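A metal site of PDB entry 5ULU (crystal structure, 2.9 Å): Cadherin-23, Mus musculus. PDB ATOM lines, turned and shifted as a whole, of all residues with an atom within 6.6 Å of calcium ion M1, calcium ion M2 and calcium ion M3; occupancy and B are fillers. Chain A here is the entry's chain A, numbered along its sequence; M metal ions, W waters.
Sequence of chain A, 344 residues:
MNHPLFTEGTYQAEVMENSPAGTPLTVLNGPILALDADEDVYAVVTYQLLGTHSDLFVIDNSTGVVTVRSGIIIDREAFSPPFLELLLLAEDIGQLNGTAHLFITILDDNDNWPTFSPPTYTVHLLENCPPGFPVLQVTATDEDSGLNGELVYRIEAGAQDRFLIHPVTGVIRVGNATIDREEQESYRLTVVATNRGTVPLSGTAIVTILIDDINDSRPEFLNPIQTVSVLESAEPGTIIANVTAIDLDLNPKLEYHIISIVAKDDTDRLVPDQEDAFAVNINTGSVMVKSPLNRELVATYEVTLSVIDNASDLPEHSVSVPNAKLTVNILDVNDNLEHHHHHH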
ATOM      1  N   GLU A 127      19.555 -30.399  18.077  1.00  0.00           N
ATOM      2  CA  GLU A 127      19.424 -29.098  17.403  1.00  0.00           C
ATOM      3  C   GLU A 127      19.952 -29.108  15.958  1.00  0.00           C
ATOM      4  O   GLU A 127      20.527 -30.107  15.480  1.00  0.00           O
ATOM      5  CB  GLU A 127      20.079 -27.963  18.226  1.00  0.00           C
ATOM      6  CG  GLU A 127      21.590 -28.059  18.418  1.00  0.00           C
ATOM      7  CD  GLU A 127      22.209 -26.775  18.983  1.00  0.00           C
ATOM      8  OE1 GLU A 127      23.069 -26.866  19.871  1.00  0.00           O
ATOM      9  OE2 GLU A 127      21.844 -25.659  18.558  1.00  0.00           O
ATOM     10  N   ASN A 128      19.688 -28.002  15.256  1.00  0.00           N
ATOM     11  CA  ASN A 128      20.112 -27.811  13.850  1.00  0.00           C
ATOM     12  C   ASN A 128      19.569 -28.847  12.894  1.00  0.00           C
ATOM     13  O   ASN A 128      20.133 -29.061  11.811  1.00  0.00           O
ATOM     14  CB  ASN A 128      21.635 -27.798  13.735  1.00  0.00           C
ATOM     15  CG  ASN A 128      22.288 -26.863  14.709  1.00  0.00           C
ATOM     16  OD1 ASN A 128      21.696 -25.879  15.186  1.00  0.00           O
ATOM     17  ND2 ASN A 128      23.545 -27.164  15.002  1.00  0.00           N
ATOM     18  N   ILE A 179      16.007 -24.634  14.444  1.00  0.00           N
ATOM     19  CA  ILE A 179      15.777 -24.850  15.850  1.00  0.00           C
ATOM     20  C   ILE A 179      17.160 -24.918  16.525  1.00  0.00           C
ATOM     21  O   ILE A 179      17.902 -25.904  16.448  1.00  0.00           O
ATOM     22  CB  ILE A 179      14.789 -26.023  16.118  1.00  0.00           C
ATOM     23  CG1 ILE A 179      15.371 -27.377  15.747  1.00  0.00           C
ATOM     24  CG2 ILE A 179      13.469 -25.800  15.377  1.00  0.00           C
ATOM     25  CD1 ILE A 179      15.842 -28.161  16.966  1.00  0.00           C
ATOM     26  N   ASP A 180      17.521 -23.779  17.093  1.00  0.00           N
ATOM     27  CA  ASP A 180      18.802 -23.576  17.766  1.00  0.00           C
ATOM     28  C   ASP A 180      18.579 -23.729  19.261  1.00  0.00           C
ATOM     29  O   ASP A 180      17.698 -23.062  19.831  1.00  0.00           O
ATOM     30  CB  ASP A 180      19.279 -22.160  17.452  1.00  0.00           C
ATOM     31  CG  ASP A 180      20.646 -21.853  17.997  1.00  0.00           C
ATOM     32  OD1 ASP A 180      21.392 -22.798  18.325  1.00  0.00           O
ATOM     33  OD2 ASP A 180      20.992 -20.645  18.060  1.00  0.00           O
ATOM     34  N   ARG A 181      19.350 -24.602  19.922  1.00  0.00           N
ATOM     35  CA  ARG A 181      19.226 -24.724  21.376  1.00  0.00           C
ATOM     36  C   ARG A 181      19.549 -23.390  22.098  1.00  0.00           C
ATOM     37  O   ARG A 181      18.876 -23.011  23.051  1.00  0.00           O
ATOM     38  CB  ARG A 181      20.097 -25.851  21.920  1.00  0.00           C
ATOM     39  CG  ARG A 181      19.601 -26.381  23.284  1.00  0.00           C
ATOM     40  CD  ARG A 181      20.663 -27.187  23.988  1.00  0.00           C
ATOM     41  NE  ARG A 181      21.779 -26.315  24.323  1.00  0.00           N
ATOM     42  CZ  ARG A 181      21.799 -25.481  25.357  1.00  0.00           C
ATOM     43  NH1 ARG A 181      20.786 -25.429  26.207  1.00  0.00           N
ATOM     44  NH2 ARG A 181      22.859 -24.696  25.527  1.00  0.00           N
ATOM     45  N   GLU A 182      20.544 -22.665  21.594  1.00  0.00           N
ATOM     46  CA  GLU A 182      20.984 -21.429  22.214  1.00  0.00           C
ATOM     47  C   GLU A 182      19.995 -20.268  21.990  1.00  0.00           C
ATOM     48  O   GLU A 182      20.142 -19.205  22.611  1.00  0.00           O
ATOM     49  CB  GLU A 182      22.379 -21.036  21.715  1.00  0.00           C
ATOM     50  CG  GLU A 182      23.528 -21.911  22.198  1.00  0.00           C
ATOM     51  CD  GLU A 182      23.557 -23.308  21.597  1.00  0.00           C
ATOM     52  OE1 GLU A 182      24.012 -24.242  22.267  1.00  0.00           O
ATOM     53  OE2 GLU A 182      23.133 -23.515  20.443  1.00  0.00           O
ATOM     54  N   GLU A 183      19.022 -20.464  21.106  1.00  0.00           N
ATOM     55  CA  GLU A 183      17.876 -19.538  20.916  1.00  0.00           C
ATOM     56  C   GLU A 183      16.775 -19.848  21.913  1.00  0.00           C
ATOM     57  O   GLU A 183      16.218 -18.958  22.525  1.00  0.00           O
ATOM     58  CB  GLU A 183      17.339 -19.663  19.474  1.00  0.00           C
ATOM     59  CG  GLU A 183      16.028 -18.973  19.100  1.00  0.00           C
ATOM     60  CD  GLU A 183      15.526 -19.465  17.735  1.00  0.00           C
ATOM     61  OE1 GLU A 183      15.522 -18.641  16.788  1.00  0.00           O
ATOM     62  OE2 GLU A 183      15.187 -20.685  17.612  1.00  0.00           O
ATOM     63  N   ASP A 212      18.179 -31.089  22.720  1.00  0.00           N
ATOM     64  CA  ASP A 212      19.521 -31.554  23.064  1.00  0.00           C
ATOM     65  C   ASP A 212      20.571 -30.693  22.396  1.00  0.00           C
ATOM     66  O   ASP A 212      20.292 -30.020  21.414  1.00  0.00           O
ATOM     67  CB  ASP A 212      19.691 -33.029  22.710  1.00  0.00           C
ATOM     68  CG  ASP A 212      18.883 -33.953  23.597  1.00  0.00           C
ATOM     69  OD1 ASP A 212      18.100 -33.456  24.459  1.00  0.00           O
ATOM     70  OD2 ASP A 212      19.029 -35.183  23.456  1.00  0.00           O
ATOM     71  N   ASP A 213      21.783 -30.726  22.929  1.00  0.00           N
ATOM     72  CA  ASP A 213      22.819 -29.798  22.525  1.00  0.00           C
ATOM     73  C   ASP A 213      23.790 -30.394  21.527  1.00  0.00           C
ATOM     74  O   ASP A 213      24.180 -31.557  21.618  1.00  0.00           O
ATOM     75  CB  ASP A 213      23.623 -29.332  23.748  1.00  0.00           C
ATOM     76  CG  ASP A 213      24.593 -28.196  23.421  1.00  0.00           C
ATOM     77  OD1 ASP A 213      24.125 -27.178  22.866  1.00  0.00           O
ATOM     78  OD2 ASP A 213      25.819 -28.334  23.721  1.00  0.00           O
ATOM     79  N   ILE A 214      24.153 -29.551  20.568  1.00  0.00           N
ATOM     80  CA  ILE A 214      25.352 -29.714  19.785  1.00  0.00           C
ATOM     81  C   ILE A 214      26.242 -28.544  20.197  1.00  0.00           C
ATOM     82  O   ILE A 214      25.746 -27.410  20.322  1.00  0.00           O
ATOM     83  CB  ILE A 214      25.037 -29.646  18.273  1.00  0.00           C
ATOM     84  CG1 ILE A 214      24.120 -30.804  17.860  1.00  0.00           C
ATOM     85  CG2 ILE A 214      26.323 -29.722  17.452  1.00  0.00           C
ATOM     86  CD1 ILE A 214      23.739 -30.801  16.397  1.00  0.00           C
ATOM     87  N   ASN A 215      27.531 -28.815  20.415  1.00  0.00           N
ATOM     88  CA  ASN A 215      28.499 -27.741  20.651  1.00  0.00           C
ATOM     89  C   ASN A 215      28.785 -27.050  19.311  1.00  0.00           C
ATOM     90  O   ASN A 215      29.744 -27.382  18.563  1.00  0.00           O
ATOM     91  CB  ASN A 215      29.755 -28.267  21.328  1.00  0.00           C
ATOM     92  CG  ASN A 215      30.687 -27.157  21.747  1.00  0.00           C
ATOM     93  OD1 ASN A 215      30.493 -26.006  21.376  1.00  0.00           O
ATOM     94  ND2 ASN A 215      31.712 -27.500  22.503  1.00  0.00           N
ATOM     95  N   ASP A 216      27.912 -26.101  19.005  1.00  0.00           N
ATOM     96  CA  ASP A 216      27.840 -25.511  17.675  1.00  0.00           C
ATOM     97  C   ASP A 216      28.013 -24.004  17.689  1.00  0.00           C
ATOM     98  O   ASP A 216      27.878 -23.367  16.648  1.00  0.00           O
ATOM     99  CB  ASP A 216      26.510 -25.915  16.998  1.00  0.00           C
ATOM    100  CG  ASP A 216      25.281 -25.253  17.628  1.00  0.00           C
ATOM    101  OD1 ASP A 216      25.351 -24.697  18.735  1.00  0.00           O
ATOM    102  OD2 ASP A 216      24.200 -25.266  16.992  1.00  0.00           O
ATOM    103  N   SER A 217      28.354 -23.443  18.860  1.00  0.00           N
ATOM    104  CA  SER A 217      28.574 -21.997  19.004  1.00  0.00           C
ATOM    105  C   SER A 217      30.044 -21.606  19.106  1.00  0.00           C
ATOM    106  O   SER A 217      30.924 -22.402  19.500  1.00  0.00           O
ATOM    107  CB  SER A 217      27.832 -21.413  20.201  1.00  0.00           C
ATOM    108  OG  SER A 217      26.465 -21.436  19.915  1.00  0.00           O
ATOM    109  N   ARG A 218      30.266 -20.356  18.754  1.00  0.00           N
ATOM    110  CA  ARG A 218      31.571 -19.761  18.711  1.00  0.00           C
ATOM    111  C   ARG A 218      31.821 -19.162  20.084  1.00  0.00           C
ATOM    112  O   ARG A 218      30.971 -18.436  20.583  1.00  0.00           O
ATOM    113  CB  ARG A 218      31.569 -18.670  17.632  1.00  0.00           C
ATOM    114  CG  ARG A 218      32.920 -18.256  17.112  1.00  0.00           C
ATOM    115  CD  ARG A 218      32.775 -17.294  15.944  1.00  0.00           C
ATOM    116  NE  ARG A 218      32.238 -17.930  14.733  1.00  0.00           N
ATOM    117  CZ  ARG A 218      32.881 -18.815  13.971  1.00  0.00           C
ATOM    118  NH1 ARG A 218      32.257 -19.328  12.907  1.00  0.00           N
ATOM    119  NH2 ARG A 218      34.130 -19.209  14.230  1.00  0.00           N
ATOM    120  N   PRO A 219      32.984 -19.466  20.700  1.00  0.00           N
ATOM    121  CA  PRO A 219      33.341 -18.648  21.849  1.00  0.00           C
ATOM    122  C   PRO A 219      33.484 -17.237  21.379  1.00  0.00           C
ATOM    123  O   PRO A 219      34.032 -17.040  20.318  1.00  0.00           O
ATOM    124  CB  PRO A 219      34.711 -19.187  22.246  1.00  0.00           C
ATOM    125  CG  PRO A 219      35.255 -19.808  21.007  1.00  0.00           C
ATOM    126  CD  PRO A 219      34.067 -20.392  20.317  1.00  0.00           C
ATOM    127  N   ASP A 247      31.066 -19.045  25.781  1.00  0.00           N
ATOM    128  CA  ASP A 247      30.565 -19.950  24.748  1.00  0.00           C
ATOM    129  C   ASP A 247      29.263 -20.527  25.245  1.00  0.00           C
ATOM    130  O   ASP A 247      29.243 -21.306  26.182  1.00  0.00           O
ATOM    131  CB  ASP A 247      31.573 -21.080  24.449  1.00  0.00           C
ATOM    132  CG  ASP A 247      31.162 -21.925  23.237  1.00  0.00           C
ATOM    133  OD1 ASP A 247      30.847 -21.357  22.194  1.00  0.00           O
ATOM    134  OD2 ASP A 247      31.138 -23.156  23.330  1.00  0.00           O
ATOM    135  N   LEU A 248      28.173 -20.187  24.562  1.00  0.00           N
ATOM    136  CA  LEU A 248      26.820 -20.472  25.003  1.00  0.00           C
ATOM    137  C   LEU A 248      26.347 -21.926  24.915  1.00  0.00           C
ATOM    138  O   LEU A 248      25.201 -22.221  25.233  1.00  0.00           O
ATOM    139  CB  LEU A 248      25.813 -19.561  24.267  1.00  0.00           C
ATOM    140  CG  LEU A 248      25.776 -18.049  24.600  1.00  0.00           C
ATOM    141  CD1 LEU A 248      24.340 -17.540  24.540  1.00  0.00           C
ATOM    142  CD2 LEU A 248      26.351 -17.704  25.977  1.00  0.00           C
ATOM    143  N   ASP A 249      27.210 -22.846  24.527  1.00  0.00           N
ATOM    144  CA  ASP A 249      26.855 -24.257  24.582  1.00  0.00           C
ATOM    145  C   ASP A 249      27.002 -24.782  26.004  1.00  0.00           C
ATOM    146  O   ASP A 249      27.638 -24.147  26.854  1.00  0.00           O
ATOM    147  CB  ASP A 249      27.770 -25.057  23.652  1.00  0.00           C
ATOM    148  CG  ASP A 249      27.704 -24.584  22.199  1.00  0.00           C
ATOM    149  OD1 ASP A 249      26.599 -24.690  21.593  1.00  0.00           O
ATOM    150  OD2 ASP A 249      28.752 -24.119  21.665  1.00  0.00           O
ATOM    151  N   LEU A 250      26.409 -25.946  26.230  1.00  0.00           N
ATOM    152  CA  LEU A 250      26.729 -26.809  27.389  1.00  0.00           C
ATOM    153  C   LEU A 250      28.200 -27.280  27.338  1.00  0.00           C
ATOM    154  O   LEU A 250      28.723 -27.616  26.266  1.00  0.00           O
ATOM    155  CB  LEU A 250      25.835 -28.048  27.391  1.00  0.00           C
ATOM    156  CG  LEU A 250      24.446 -28.017  28.036  1.00  0.00           C
ATOM    157  CD1 LEU A 250      23.708 -26.714  27.776  1.00  0.00           C
ATOM    158  CD2 LEU A 250      23.623 -29.229  27.589  1.00  0.00           C
ATOM    159  N   PRO A 252      31.403 -26.153  27.403  1.00  0.00           N
ATOM    160  CA  PRO A 252      32.524 -25.664  26.603  1.00  0.00           C
ATOM    161  C   PRO A 252      33.786 -25.766  27.426  1.00  0.00           C
ATOM    162  O   PRO A 252      33.700 -25.718  28.646  1.00  0.00           O
ATOM    163  CB  PRO A 252      32.180 -24.202  26.386  1.00  0.00           C
ATOM    164  CG  PRO A 252      31.410 -23.811  27.603  1.00  0.00           C
ATOM    165  CD  PRO A 252      30.721 -25.054  28.094  1.00  0.00           C
ATOM    166  N   LEU A 254      37.213 -23.613  27.014  1.00  0.00           N
ATOM    167  CA  LEU A 254      37.944 -22.594  26.304  1.00  0.00           C
ATOM    168  C   LEU A 254      39.407 -22.604  26.690  1.00  0.00           C
ATOM    169  O   LEU A 254      39.756 -22.986  27.814  1.00  0.00           O
ATOM    170  CB  LEU A 254      37.380 -21.209  26.634  1.00  0.00           C
ATOM    171  CG  LEU A 254      35.860 -20.968  26.599  1.00  0.00           C
ATOM    172  CD1 LEU A 254      35.537 -19.481  26.738  1.00  0.00           C
ATOM    173  CD2 LEU A 254      35.245 -21.520  25.335  1.00  0.00           C
ATOM    174  N   ASP A 309      37.073 -22.948  21.898  1.00  0.00           N
ATOM    175  CA  ASP A 309      36.313 -23.941  22.624  1.00  0.00           C
ATOM    176  C   ASP A 309      36.780 -25.292  22.118  1.00  0.00           C
ATOM    177  O   ASP A 309      36.532 -25.636  20.971  1.00  0.00           O
ATOM    178  CB  ASP A 309      34.818 -23.748  22.393  1.00  0.00           C
ATOM    179  CG  ASP A 309      33.991 -24.930  22.880  1.00  0.00           C
ATOM    180  OD1 ASP A 309      34.515 -25.785  23.642  1.00  0.00           O
ATOM    181  OD2 ASP A 309      32.820 -25.011  22.459  1.00  0.00           O
ATOM    182  N   ALA A 311      35.879 -28.310  22.866  1.00  0.00           N
ATOM    183  CA  ALA A 311      34.908 -29.396  22.833  1.00  0.00           C
ATOM    184  C   ALA A 311      33.965 -29.294  21.619  1.00  0.00           C
ATOM    185  O   ALA A 311      32.942 -29.991  21.552  1.00  0.00           O
ATOM    186  CB  ALA A 311      34.126 -29.398  24.128  1.00  0.00           C
ATOM    187  N   SER A 312      34.314 -28.433  20.650  1.00  0.00           N
ATOM    188  CA  SER A 312      33.359 -28.006  19.635  1.00  0.00           C
ATOM    189  C   SER A 312      33.194 -29.108  18.611  1.00  0.00           C
ATOM    190  O   SER A 312      34.179 -29.707  18.168  1.00  0.00           O
ATOM    191  CB  SER A 312      33.767 -26.672  18.992  1.00  0.00           C
ATOM    192  OG  SER A 312      32.641 -25.969  18.476  1.00  0.00           O
ATOM    193  N   ASP A 313      31.948 -29.394  18.275  1.00  0.00           N
ATOM    194  CA  ASP A 313      31.590 -30.472  17.328  1.00  0.00           C
ATOM    195  C   ASP A 313      31.740 -30.030  15.882  1.00  0.00           C
ATOM    196  O   ASP A 313      31.700 -30.858  14.995  1.00  0.00           O
ATOM    197  CB  ASP A 313      30.140 -30.906  17.564  1.00  0.00           C
ATOM    198  CG  ASP A 313      29.917 -31.467  18.963  1.00  0.00           C
ATOM    199  OD1 ASP A 313      30.699 -32.369  19.357  1.00  0.00           O
ATOM    200  OD2 ASP A 313      28.965 -31.025  19.654  1.00  0.00           O
ATOM    201  N   HIS A 317      32.877 -23.573  13.747  1.00  0.00           N
ATOM    202  CA  HIS A 317      32.378 -22.713  14.834  1.00  0.00           C
ATOM    203  C   HIS A 317      33.219 -22.726  16.124  1.00  0.00           C
ATOM    204  O   HIS A 317      32.750 -22.278  17.157  1.00  0.00           O
ATOM    205  CB  HIS A 317      30.918 -23.098  15.157  1.00  0.00           C
ATOM    206  CG  HIS A 317      29.946 -22.677  14.105  1.00  0.00           C
ATOM    207  ND1 HIS A 317      30.028 -21.461  13.466  1.00  0.00           N
ATOM    208  CD2 HIS A 317      28.860 -23.292  13.608  1.00  0.00           C
ATOM    209  CE1 HIS A 317      29.036 -21.353  12.600  1.00  0.00           C
ATOM    210  NE2 HIS A 317      28.312 -22.451  12.674  1.00  0.00           N
ATOM    211  N   SER A 318      34.452 -23.189  16.054  1.00  0.00           N
ATOM    212  CA  SER A 318      35.184 -23.501  17.271  1.00  0.00           C
ATOM    213  C   SER A 318      36.175 -22.421  17.715  1.00  0.00           C
ATOM    214  O   SER A 318      36.939 -22.678  18.624  1.00  0.00           O
ATOM    215  CB  SER A 318      35.905 -24.836  17.123  1.00  0.00           C
ATOM    216  OG  SER A 318      37.154 -24.671  16.495  1.00  0.00           O
HETATM  217 CA    CA M   1      24.635 -25.734  21.019  1.00  0.00          CA
HETATM  218 CA    CA M   2      23.185 -23.582  18.070  1.00  0.00          CA
HETATM  219 CA    CA M   3      31.288 -23.986  21.292  1.00  0.00          CA
HETATM  220  O   HOH W   1      21.958 -22.565  15.200  1.00  0.00           O
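The side-chain carboxylate (OE1) of Glu 182 sits close to the guanidinium group (NH2) of Arg 181 (3.5 Å). The side-chain hydroxyl (OG) of Ser 312 lies within hydrogen-bond range of the backbone carbonyl oxygen (O) of Asn 215 (3.2 Å). The backbone carbonyl oxygen (O) of Ala 311 lies within hydrogen-bond range of the side-chain amide nitrogen (ND2) of Asn 215, 2.9 Å away. OD2 of Asp 313 sits at hydrogen-bond distance from N of Asn 215, 2.7 Å away. The backbone NH (N) of Asp 309 lies within hydrogen-bond range of the backbone carbonyl oxygen (O) of Ser 318 (3.3 Å). The side-chain carboxylate of Asp 216 lies close to the side-chain amide nitrogen of Asn 128 (2.8 Å). The side-chain carboxylate (OE2) of Glu 127 sits close to the backbone NH (N) of Arg 181, 3.0 Å away. The side-chain carboxylate (OD1) of Asp 213 lies close to the guanidinium group (NE) of Arg 181 (2.9 Å).
Six residues have an atom within 4 Å of calcium ion M1: Glu 127, Glu 182, Asp 213, Ile 214, Asp 216 and Asp 249.
Merely in contact with calcium ion M2: Asn 128.
OG of Ser 312 touches calcium ion M3, at 3.7 Å. Six residues have an atom within 4 Å of calcium ion M3: Asn 215, Ser 217, Asp 247, Asp 249, Asp 309 and Ser 312. The nearest printed residue that does not touch calcium ion M3 is Arg 218 (4.5 Å).
Calcium ion M1 is bound by the side-chain carboxylate (OE1) of Glu 182 (2.0 Å), the backbone carbonyl oxygen (O) of Ile 214 (2.1 Å), the side-chain carboxylate (OE1) of Glu 127 (2.2 Å), the side-chain carboxylate (OD1) of Asp 249 (2.3 Å), the side-chain carboxylate (OD1) of Asp 213 (2.4 Å), the side-chain carboxylate (OD1) of Asp 216 (2.6 Å) and the side-chain carboxylate (OE2) of Glu 182 (2.7 Å).
The side-chain carboxylate (OD1) of Asp 180 binds calcium ion M2. OD2 of Asp 216 binds calcium ion M2, 2.2 Å away. The side-chain carboxylate (OE2) of Glu 182 binds calcium ion M2 (2.4 Å). OE2 of Glu 127 is bound to calcium ion M2, at 2.5 Å. OD1 of Asp 216 binds calcium ion M2 (2.5 Å).
Calcium ion M3 is bound by OD1 of Asn 215, OD2 of Asp 309, OD2 of Asp 247, O of Ser 217, OD2 of Asp 249 and OD1 of Asp 247. Calcium ion M3 has six donor atoms within binding distance.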
